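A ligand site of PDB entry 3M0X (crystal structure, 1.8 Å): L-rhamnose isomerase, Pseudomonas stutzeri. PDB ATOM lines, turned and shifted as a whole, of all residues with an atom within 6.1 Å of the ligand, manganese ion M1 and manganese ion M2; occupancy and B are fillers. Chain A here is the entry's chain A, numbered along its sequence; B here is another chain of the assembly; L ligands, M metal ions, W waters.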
ATOM      1  N   TRP A  57     -20.034  14.684   4.224  1.00  0.00           N
ATOM      2  CA  TRP A  57     -20.013  14.128   2.870  1.00  0.00           C
ATOM      3  C   TRP A  57     -20.998  12.986   2.662  1.00  0.00           C
ATOM      4  O   TRP A  57     -21.129  12.466   1.546  1.00  0.00           O
ATOM      5  CB  TRP A  57     -18.587  13.684   2.523  1.00  0.00           C
ATOM      6  CG  TRP A  57     -18.056  12.589   3.390  1.00  0.00           C
ATOM      7  CD1 TRP A  57     -18.171  11.247   3.176  1.00  0.00           C
ATOM      8  CD2 TRP A  57     -17.315  12.742   4.605  1.00  0.00           C
ATOM      9  NE1 TRP A  57     -17.531  10.552   4.173  1.00  0.00           N
ATOM     10  CE2 TRP A  57     -17.003  11.444   5.065  1.00  0.00           C
ATOM     11  CE3 TRP A  57     -16.885  13.847   5.342  1.00  0.00           C
ATOM     12  CZ2 TRP A  57     -16.276  11.213   6.239  1.00  0.00           C
ATOM     13  CZ3 TRP A  57     -16.158  13.616   6.517  1.00  0.00           C
ATOM     14  CH2 TRP A  57     -15.864  12.314   6.945  1.00  0.00           C
ATOM     15  N   HIS A 101     -14.927  17.959   6.092  1.00  0.00           N
ATOM     16  CA  HIS A 101     -13.910  17.523   5.142  1.00  0.00           C
ATOM     17  C   HIS A 101     -13.469  18.762   4.369  1.00  0.00           C
ATOM     18  O   HIS A 101     -14.290  19.469   3.778  1.00  0.00           O
ATOM     19  CB  HIS A 101     -14.468  16.463   4.193  1.00  0.00           C
ATOM     20  CG  HIS A 101     -13.493  15.379   3.872  1.00  0.00           C
ATOM     21  ND1 HIS A 101     -12.355  15.593   3.129  1.00  0.00           N
ATOM     22  CD2 HIS A 101     -13.482  14.062   4.196  1.00  0.00           C
ATOM     23  CE1 HIS A 101     -11.680  14.456   3.015  1.00  0.00           C
ATOM     24  NE2 HIS A 101     -12.350  13.507   3.658  1.00  0.00           N
ATOM     25  N   TRP A 104     -13.769  20.326   0.750  1.00  0.00           N
ATOM     26  CA  TRP A 104     -15.184  20.220   0.379  1.00  0.00           C
ATOM     27  C   TRP A 104     -16.052  21.159   1.202  1.00  0.00           C
ATOM     28  O   TRP A 104     -16.904  21.860   0.646  1.00  0.00           O
ATOM     29  CB  TRP A 104     -15.711  18.793   0.549  1.00  0.00           C
ATOM     30  CG  TRP A 104     -15.071  17.762  -0.327  1.00  0.00           C
ATOM     31  CD1 TRP A 104     -14.412  17.973  -1.506  1.00  0.00           C
ATOM     32  CD2 TRP A 104     -15.048  16.343  -0.095  1.00  0.00           C
ATOM     33  NE1 TRP A 104     -13.973  16.771  -2.018  1.00  0.00           N
ATOM     34  CE2 TRP A 104     -14.343  15.757  -1.173  1.00  0.00           C
ATOM     35  CE3 TRP A 104     -15.539  15.518   0.922  1.00  0.00           C
ATOM     36  CZ2 TRP A 104     -14.135  14.376  -1.276  1.00  0.00           C
ATOM     37  CZ3 TRP A 104     -15.332  14.151   0.824  1.00  0.00           C
ATOM     38  CH2 TRP A 104     -14.636  13.591  -0.265  1.00  0.00           C
ATOM     39  N   ASN A 127     -11.108  16.413   8.638  1.00  0.00           N
ATOM     40  CA  ASN A 127     -10.606  15.453   7.658  1.00  0.00           C
ATOM     41  C   ASN A 127      -9.938  16.229   6.543  1.00  0.00           C
ATOM     42  O   ASN A 127     -10.551  17.117   5.946  1.00  0.00           O
ATOM     43  CB  ASN A 127     -11.767  14.646   7.081  1.00  0.00           C
ATOM     44  CG  ASN A 127     -12.452  13.804   8.131  1.00  0.00           C
ATOM     45  OD1 ASN A 127     -12.071  12.657   8.367  1.00  0.00           O
ATOM     46  ND2 ASN A 127     -13.466  14.362   8.771  1.00  0.00           N
ATOM     47  N   SER A 128      -8.676  15.896   6.271  1.00  0.00           N
ATOM     48  CA  SER A 128      -7.928  16.556   5.211  1.00  0.00           C
ATOM     49  C   SER A 128      -8.147  15.829   3.893  1.00  0.00           C
ATOM     50  O   SER A 128      -8.581  14.676   3.880  1.00  0.00           O
ATOM     51  CB  SER A 128      -6.431  16.562   5.554  1.00  0.00           C
ATOM     52  OG  SER A 128      -5.947  15.249   5.779  1.00  0.00           O
ATOM     53  N   PHE A 131      -6.061  13.518  -1.675  1.00  0.00           N
ATOM     54  CA  PHE A 131      -6.279  12.387  -2.570  1.00  0.00           C
ATOM     55  C   PHE A 131      -6.993  12.864  -3.840  1.00  0.00           C
ATOM     56  O   PHE A 131      -7.468  12.071  -4.650  1.00  0.00           O
ATOM     57  CB  PHE A 131      -7.086  11.287  -1.854  1.00  0.00           C
ATOM     58  CG  PHE A 131      -8.357  11.767  -1.206  1.00  0.00           C
ATOM     59  CD1 PHE A 131      -9.489  12.054  -1.968  1.00  0.00           C
ATOM     60  CD2 PHE A 131      -8.412  11.943   0.177  1.00  0.00           C
ATOM     61  CE1 PHE A 131     -10.655  12.498  -1.358  1.00  0.00           C
ATOM     62  CE2 PHE A 131      -9.585  12.393   0.790  1.00  0.00           C
ATOM     63  CZ  PHE A 131     -10.703  12.668   0.021  1.00  0.00           C
ATOM     64  N   THR A 177      -8.135  13.825  11.185  1.00  0.00           N
ATOM     65  CA  THR A 177      -8.054  12.482  10.642  1.00  0.00           C
ATOM     66  C   THR A 177      -7.388  12.586   9.283  1.00  0.00           C
ATOM     67  O   THR A 177      -7.774  13.420   8.461  1.00  0.00           O
ATOM     68  CB  THR A 177      -9.430  11.861  10.465  1.00  0.00           C
ATOM     69  OG1 THR A 177     -10.043  11.708  11.755  1.00  0.00           O
ATOM     70  CG2 THR A 177      -9.327  10.498   9.793  1.00  0.00           C
ATOM     71  N   TRP A 179      -6.472  10.488   5.939  1.00  0.00           N
ATOM     72  CA  TRP A 179      -6.585   9.320   5.068  1.00  0.00           C
ATOM     73  C   TRP A 179      -6.111   9.804   3.704  1.00  0.00           C
ATOM     74  O   TRP A 179      -6.587  10.821   3.198  1.00  0.00           O
ATOM     75  CB  TRP A 179      -8.025   8.824   4.914  1.00  0.00           C
ATOM     76  CG  TRP A 179      -8.077   7.733   3.880  1.00  0.00           C
ATOM     77  CD1 TRP A 179      -7.553   6.478   3.992  1.00  0.00           C
ATOM     78  CD2 TRP A 179      -8.505   7.861   2.518  1.00  0.00           C
ATOM     79  NE1 TRP A 179      -7.607   5.821   2.784  1.00  0.00           N
ATOM     80  CE2 TRP A 179      -8.196   6.646   1.870  1.00  0.00           C
ATOM     81  CE3 TRP A 179      -9.115   8.889   1.788  1.00  0.00           C
ATOM     82  CZ2 TRP A 179      -8.478   6.436   0.513  1.00  0.00           C
ATOM     83  CZ3 TRP A 179      -9.396   8.675   0.441  1.00  0.00           C
ATOM     84  CH2 TRP A 179      -9.070   7.454  -0.190  1.00  0.00           C
ATOM     85  N   GLU A 219      -5.666   6.789   9.169  1.00  0.00           N
ATOM     86  CA  GLU A 219      -6.610   5.760   8.781  1.00  0.00           C
ATOM     87  C   GLU A 219      -6.033   4.817   7.721  1.00  0.00           C
ATOM     88  O   GLU A 219      -5.681   5.246   6.623  1.00  0.00           O
ATOM     89  CB  GLU A 219      -7.884   6.438   8.257  1.00  0.00           C
ATOM     90  CG  GLU A 219      -8.958   5.508   7.731  1.00  0.00           C
ATOM     91  CD  GLU A 219     -10.219   6.249   7.303  1.00  0.00           C
ATOM     92  OE1 GLU A 219     -10.161   7.488   7.155  1.00  0.00           O
ATOM     93  OE2 GLU A 219     -11.259   5.591   7.107  1.00  0.00           O
ATOM     94  N   LYS A 221      -6.042   1.539   5.015  1.00  0.00           N
ATOM     95  CA  LYS A 221      -6.968   1.025   4.007  1.00  0.00           C
ATOM     96  C   LYS A 221      -6.181   0.084   3.099  1.00  0.00           C
ATOM     97  O   LYS A 221      -5.145   0.465   2.551  1.00  0.00           O
ATOM     98  CB  LYS A 221      -7.554   2.186   3.204  1.00  0.00           C
ATOM     99  CG  LYS A 221      -8.729   1.783   2.326  1.00  0.00           C
ATOM    100  CD  LYS A 221      -9.264   2.964   1.534  1.00  0.00           C
ATOM    101  CE  LYS A 221     -10.533   2.579   0.783  1.00  0.00           C
ATOM    102  NZ  LYS A 221     -11.028   3.717  -0.052  1.00  0.00           N
ATOM    103  N   GLU A 224      -7.558   0.897  -2.881  1.00  0.00           N
ATOM    104  CA  GLU A 224      -8.463   1.918  -3.452  1.00  0.00           C
ATOM    105  C   GLU A 224      -8.218   3.275  -2.801  1.00  0.00           C
ATOM    106  O   GLU A 224      -8.499   3.475  -1.624  1.00  0.00           O
ATOM    107  CB  GLU A 224      -9.939   1.556  -3.295  1.00  0.00           C
ATOM    108  CG  GLU A 224     -10.845   2.579  -3.994  1.00  0.00           C
ATOM    109  CD  GLU A 224     -12.311   2.451  -3.613  1.00  0.00           C
ATOM    110  OE1 GLU A 224     -12.604   2.106  -2.450  1.00  0.00           O
ATOM    111  OE2 GLU A 224     -13.161   2.729  -4.473  1.00  0.00           O
ATOM    112  N   LEU A 252      -7.110   5.084  13.409  1.00  0.00           N
ATOM    113  CA  LEU A 252      -8.539   5.115  13.176  1.00  0.00           C
ATOM    114  C   LEU A 252      -8.883   3.877  12.357  1.00  0.00           C
ATOM    115  O   LEU A 252      -8.250   3.599  11.337  1.00  0.00           O
ATOM    116  CB  LEU A 252      -8.960   6.383  12.442  1.00  0.00           C
ATOM    117  CG  LEU A 252     -10.485   6.477  12.279  1.00  0.00           C
ATOM    118  CD1 LEU A 252     -10.963   7.875  12.642  1.00  0.00           C
ATOM    119  CD2 LEU A 252     -10.863   6.107  10.857  1.00  0.00           C
ATOM    120  N   ASP A 254     -11.610   2.003  10.095  1.00  0.00           N
ATOM    121  CA  ASP A 254     -12.804   2.139   9.265  1.00  0.00           C
ATOM    122  C   ASP A 254     -13.165   0.689   8.961  1.00  0.00           C
ATOM    123  O   ASP A 254     -12.388  -0.027   8.342  1.00  0.00           O
ATOM    124  CB  ASP A 254     -12.477   2.890   7.966  1.00  0.00           C
ATOM    125  CG  ASP A 254     -13.703   3.109   7.095  1.00  0.00           C
ATOM    126  OD1 ASP A 254     -14.429   2.140   6.827  1.00  0.00           O
ATOM    127  OD2 ASP A 254     -13.929   4.262   6.667  1.00  0.00           O
ATOM    128  N   HIS A 257     -12.345  -1.201   5.535  1.00  0.00           N
ATOM    129  CA  HIS A 257     -10.991  -1.095   4.979  1.00  0.00           C
ATOM    130  C   HIS A 257     -10.079  -2.298   5.204  1.00  0.00           C
ATOM    131  O   HIS A 257      -8.860  -2.160   5.206  1.00  0.00           O
ATOM    132  CB  HIS A 257     -10.313   0.147   5.547  1.00  0.00           C
ATOM    133  CG  HIS A 257     -10.892   1.440   5.060  1.00  0.00           C
ATOM    134  ND1 HIS A 257     -10.279   2.653   5.294  1.00  0.00           N
ATOM    135  CD2 HIS A 257     -12.004   1.701   4.329  1.00  0.00           C
ATOM    136  CE1 HIS A 257     -10.987   3.611   4.725  1.00  0.00           C
ATOM    137  NE2 HIS A 257     -12.038   3.065   4.142  1.00  0.00           N
ATOM    138  N   HIS A 281     -14.666   4.520  12.141  1.00  0.00           N
ATOM    139  CA  HIS A 281     -15.410   5.013  10.989  1.00  0.00           C
ATOM    140  C   HIS A 281     -16.375   3.870  10.767  1.00  0.00           C
ATOM    141  O   HIS A 281     -15.996   2.808  10.261  1.00  0.00           O
ATOM    142  CB  HIS A 281     -14.514   5.218   9.763  1.00  0.00           C
ATOM    143  CG  HIS A 281     -14.042   6.626   9.595  1.00  0.00           C
ATOM    144  ND1 HIS A 281     -13.417   7.071   8.453  1.00  0.00           N
ATOM    145  CD2 HIS A 281     -14.104   7.689  10.431  1.00  0.00           C
ATOM    146  CE1 HIS A 281     -13.107   8.354   8.595  1.00  0.00           C
ATOM    147  NE2 HIS A 281     -13.507   8.749   9.785  1.00  0.00           N
ATOM    148  N   ASN A 283     -19.613   1.785   9.244  1.00  0.00           N
ATOM    149  CA  ASN A 283     -20.315   1.531   7.996  1.00  0.00           C
ATOM    150  C   ASN A 283     -20.378   0.021   7.875  1.00  0.00           C
ATOM    151  O   ASN A 283     -19.828  -0.691   8.707  1.00  0.00           O
ATOM    152  CB  ASN A 283     -19.558   2.130   6.794  1.00  0.00           C
ATOM    153  CG  ASN A 283     -18.091   1.718   6.754  1.00  0.00           C
ATOM    154  OD1 ASN A 283     -17.755   0.526   6.701  1.00  0.00           O
ATOM    155  ND2 ASN A 283     -17.209   2.705   6.781  1.00  0.00           N
ATOM    156  N   ASP A 289     -14.776  -1.718   0.158  1.00  0.00           N
ATOM    157  CA  ASP A 289     -15.090  -0.576   1.027  1.00  0.00           C
ATOM    158  C   ASP A 289     -16.418  -0.033   0.515  1.00  0.00           C
ATOM    159  O   ASP A 289     -16.501   1.075  -0.004  1.00  0.00           O
ATOM    160  CB  ASP A 289     -13.978   0.485   0.929  1.00  0.00           C
ATOM    161  CG  ASP A 289     -14.225   1.664   1.845  1.00  0.00           C
ATOM    162  OD1 ASP A 289     -14.861   1.457   2.914  1.00  0.00           O
ATOM    163  OD2 ASP A 289     -13.779   2.783   1.521  1.00  0.00           O
ATOM    164  N   ASP A 291     -19.052   1.105   1.977  1.00  0.00           N
ATOM    165  CA  ASP A 291     -19.612   2.272   2.654  1.00  0.00           C
ATOM    166  C   ASP A 291     -21.135   2.241   2.789  1.00  0.00           C
ATOM    167  O   ASP A 291     -21.794   3.250   2.597  1.00  0.00           O
ATOM    168  CB  ASP A 291     -19.191   3.549   1.920  1.00  0.00           C
ATOM    169  CG  ASP A 291     -17.757   3.912   2.187  1.00  0.00           C
ATOM    170  OD1 ASP A 291     -17.361   3.855   3.376  1.00  0.00           O
ATOM    171  OD2 ASP A 291     -17.032   4.261   1.232  1.00  0.00           O
ATOM    172  N   ASP A 327     -18.909   6.811   8.521  1.00  0.00           N
ATOM    173  CA  ASP A 327     -18.286   7.161   7.248  1.00  0.00           C
ATOM    174  C   ASP A 327     -18.988   6.295   6.229  1.00  0.00           C
ATOM    175  O   ASP A 327     -18.612   5.145   6.003  1.00  0.00           O
ATOM    176  CB  ASP A 327     -16.784   6.869   7.214  1.00  0.00           C
ATOM    177  CG  ASP A 327     -16.159   7.273   5.874  1.00  0.00           C
ATOM    178  OD1 ASP A 327     -16.891   7.813   5.027  1.00  0.00           O
ATOM    179  OD2 ASP A 327     -14.947   7.057   5.673  1.00  0.00           O
ATOM    180  N   ARG B  65     -13.492   6.610  -7.857  1.00  0.00           N
ATOM    181  CA  ARG B  65     -14.570   7.418  -7.310  1.00  0.00           C
ATOM    182  C   ARG B  65     -14.019   8.571  -6.487  1.00  0.00           C
ATOM    183  O   ARG B  65     -14.752   9.517  -6.144  1.00  0.00           O
ATOM    184  CB  ARG B  65     -15.505   6.575  -6.439  1.00  0.00           C
ATOM    185  CG  ARG B  65     -14.832   5.942  -5.242  1.00  0.00           C
ATOM    186  CD  ARG B  65     -15.859   5.358  -4.264  1.00  0.00           C
ATOM    187  NE  ARG B  65     -15.188   4.498  -3.288  1.00  0.00           N
ATOM    188  CZ  ARG B  65     -15.638   4.244  -2.059  1.00  0.00           C
ATOM    189  NH1 ARG B  65     -16.767   4.790  -1.621  1.00  0.00           N
ATOM    190  NH2 ARG B  65     -14.929   3.443  -1.261  1.00  0.00           N
ATOM    191  N   PHE B  66     -12.729   8.516  -6.179  1.00  0.00           N
ATOM    192  CA  PHE B  66     -12.087   9.558  -5.377  1.00  0.00           C
ATOM    193  C   PHE B  66     -11.547  10.714  -6.206  1.00  0.00           C
ATOM    194  O   PHE B  66     -11.615  11.862  -5.789  1.00  0.00           O
ATOM    195  CB  PHE B  66     -10.959   8.952  -4.548  1.00  0.00           C
ATOM    196  CG  PHE B  66     -11.444   8.099  -3.434  1.00  0.00           C
ATOM    197  CD1 PHE B  66     -12.037   8.680  -2.310  1.00  0.00           C
ATOM    198  CD2 PHE B  66     -11.384   6.715  -3.517  1.00  0.00           C
ATOM    199  CE1 PHE B  66     -12.546   7.900  -1.296  1.00  0.00           C
ATOM    200  CE2 PHE B  66     -11.899   5.915  -2.509  1.00  0.00           C
ATOM    201  CZ  PHE B  66     -12.479   6.513  -1.391  1.00  0.00           C
HETATM  202  C1  LIG L   1     -11.677   6.465   2.202  1.00  0.00           C
HETATM  203  O1  LIG L   1     -12.062   5.150   1.833  1.00  0.00           O
HETATM  204  C2  LIG L   1     -12.199   6.792   3.588  1.00  0.00           C
HETATM  205  O2  LIG L   1     -12.779   5.946   4.267  1.00  0.00           O
HETATM  206  C3  LIG L   1     -11.774   8.105   4.230  1.00  0.00           C
HETATM  207  O3  LIG L   1     -12.225   8.150   5.568  1.00  0.00           O
HETATM  208  C4  LIG L   1     -12.346   9.293   3.435  1.00  0.00           C
HETATM  209  O4  LIG L   1     -11.764  10.497   3.896  1.00  0.00           O
HETATM  210  C5  LIG L   1     -13.873   9.379   3.559  1.00  0.00           C
HETATM  211  O5  LIG L   1     -14.443   8.121   3.227  1.00  0.00           O
HETATM  212  C6  LIG L   1     -14.406  10.442   2.595  1.00  0.00           C
HETATM  213  O6  LIG L   1     -14.255   9.995   1.261  1.00  0.00           O
HETATM  214 MN    MN M   1     -13.189   6.288   6.481  1.00  0.00          MN
HETATM  215 MN    MN M   2     -13.280   4.270   2.946  1.00  0.00          MN
HETATM  216  O   HOH W   1     -10.777  10.978   6.473  1.00  0.00           O
HETATM  217  O   HOH W   2     -14.890   3.717   4.020  1.00  0.00           O
HETATM  218  O   HOH W   3     -14.680   5.559   1.857  1.00  0.00           O
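Manganese ion M2 is bound by O1 of the ligand, water W2, NE2 of His 257, OD2 of Asp 289, O2 of the ligand and water W3.
Manganese ion M2 has six donor atoms within binding distance.
Trp 57 touches the ligand.
Trp 104 touches the ligand (CH2 to O6, 3.9 Å).
Trp 179 touches the ligand (CD2 to C1, 3.5 Å).
Phe 66 of chain B touches the ligand (CZ to O1, 3.5 Å).
Hydrophobic or aromatic side chains within 4 Å of the ligand: Trp 57, His 101, Trp 104, Trp 179, His 257, His 281 and Phe 66 of chain B.
Within 4 Å of the ligand: Trp 57, His 101, Trp 104, Trp 179, Glu 219, Lys 221, Asp 254, His 257, His 281, Asp 289, Asp 327 and Phe 66 of chain B.
An oxygen (O1) of the ligand sits close to the side-chain amino group of Lys 221, 2.6 Å away.
A ring nitrogen (NE2) of His 101 sits at hydrogen-bond distance from an oxygen (O4) of the ligand.
The side-chain carboxylate (OD1) of Asp 327 is in hydrogen-bond range of the indole nitrogen (NE1) of Trp 57 (2.9 Å).
The backbone carbonyl oxygen (O) of Asp 327 sits at hydrogen-bond distance from the side-chain amide nitrogen (ND2) of Asn 283, at 2.9 Å.
The side-chain carboxylate (OD2) of Asp 289 lies close to the side-chain amino group (NZ) of Lys 221, 3.3 Å away.
NH2 of Arg 65 of chain B is in hydrogen-bond range of O of Asp 289 (3.1 Å).
The side-chain amide nitrogen of Asn 283 is in hydrogen-bond range of the side-chain carboxylate of Asp 254, 2.8 Å away.
OE1 of Glu 224 lies within salt-bridge range of NZ of Lys 221.
Lys 221 touches manganese ion M2 (NZ to MN, 3.8 Å).
Within 4 Å of manganese ion M2: Lys 221, Asp 254, His 257 and Asp 289.
Of the 21 residues printed, 5 come within 4 Å of manganese ion M1.
The nearest printed residue that does not touch manganese ion M1 is Leu 252 (5.0 Å).
Manganese ion M1 is bound by the side-chain carboxylate (OD2) of Asp 327 (2.1 Å), a ring nitrogen (ND1) of His 281 (2.1 Å), the side-chain carboxylate (OE2) of Glu 219 (2.1 Å), the side-chain carboxylate (OD2) of Asp 254 (2.2 Å), an oxygen (O2) of the ligand (2.3 Å) and an oxygen (O3) of the ligand (2.3 Å).
Water W3 lies within hydrogen-bond range of the side-chain carboxylate of Asp 291 (2.8 Å) and an oxygen (O5) of the ligand (2.9 Å).
Water W1 lies within hydrogen-bond range of an oxygen (O4) of the ligand (2.8 Å) and the side-chain amide oxygen of Asn 127 (2.8 Å).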
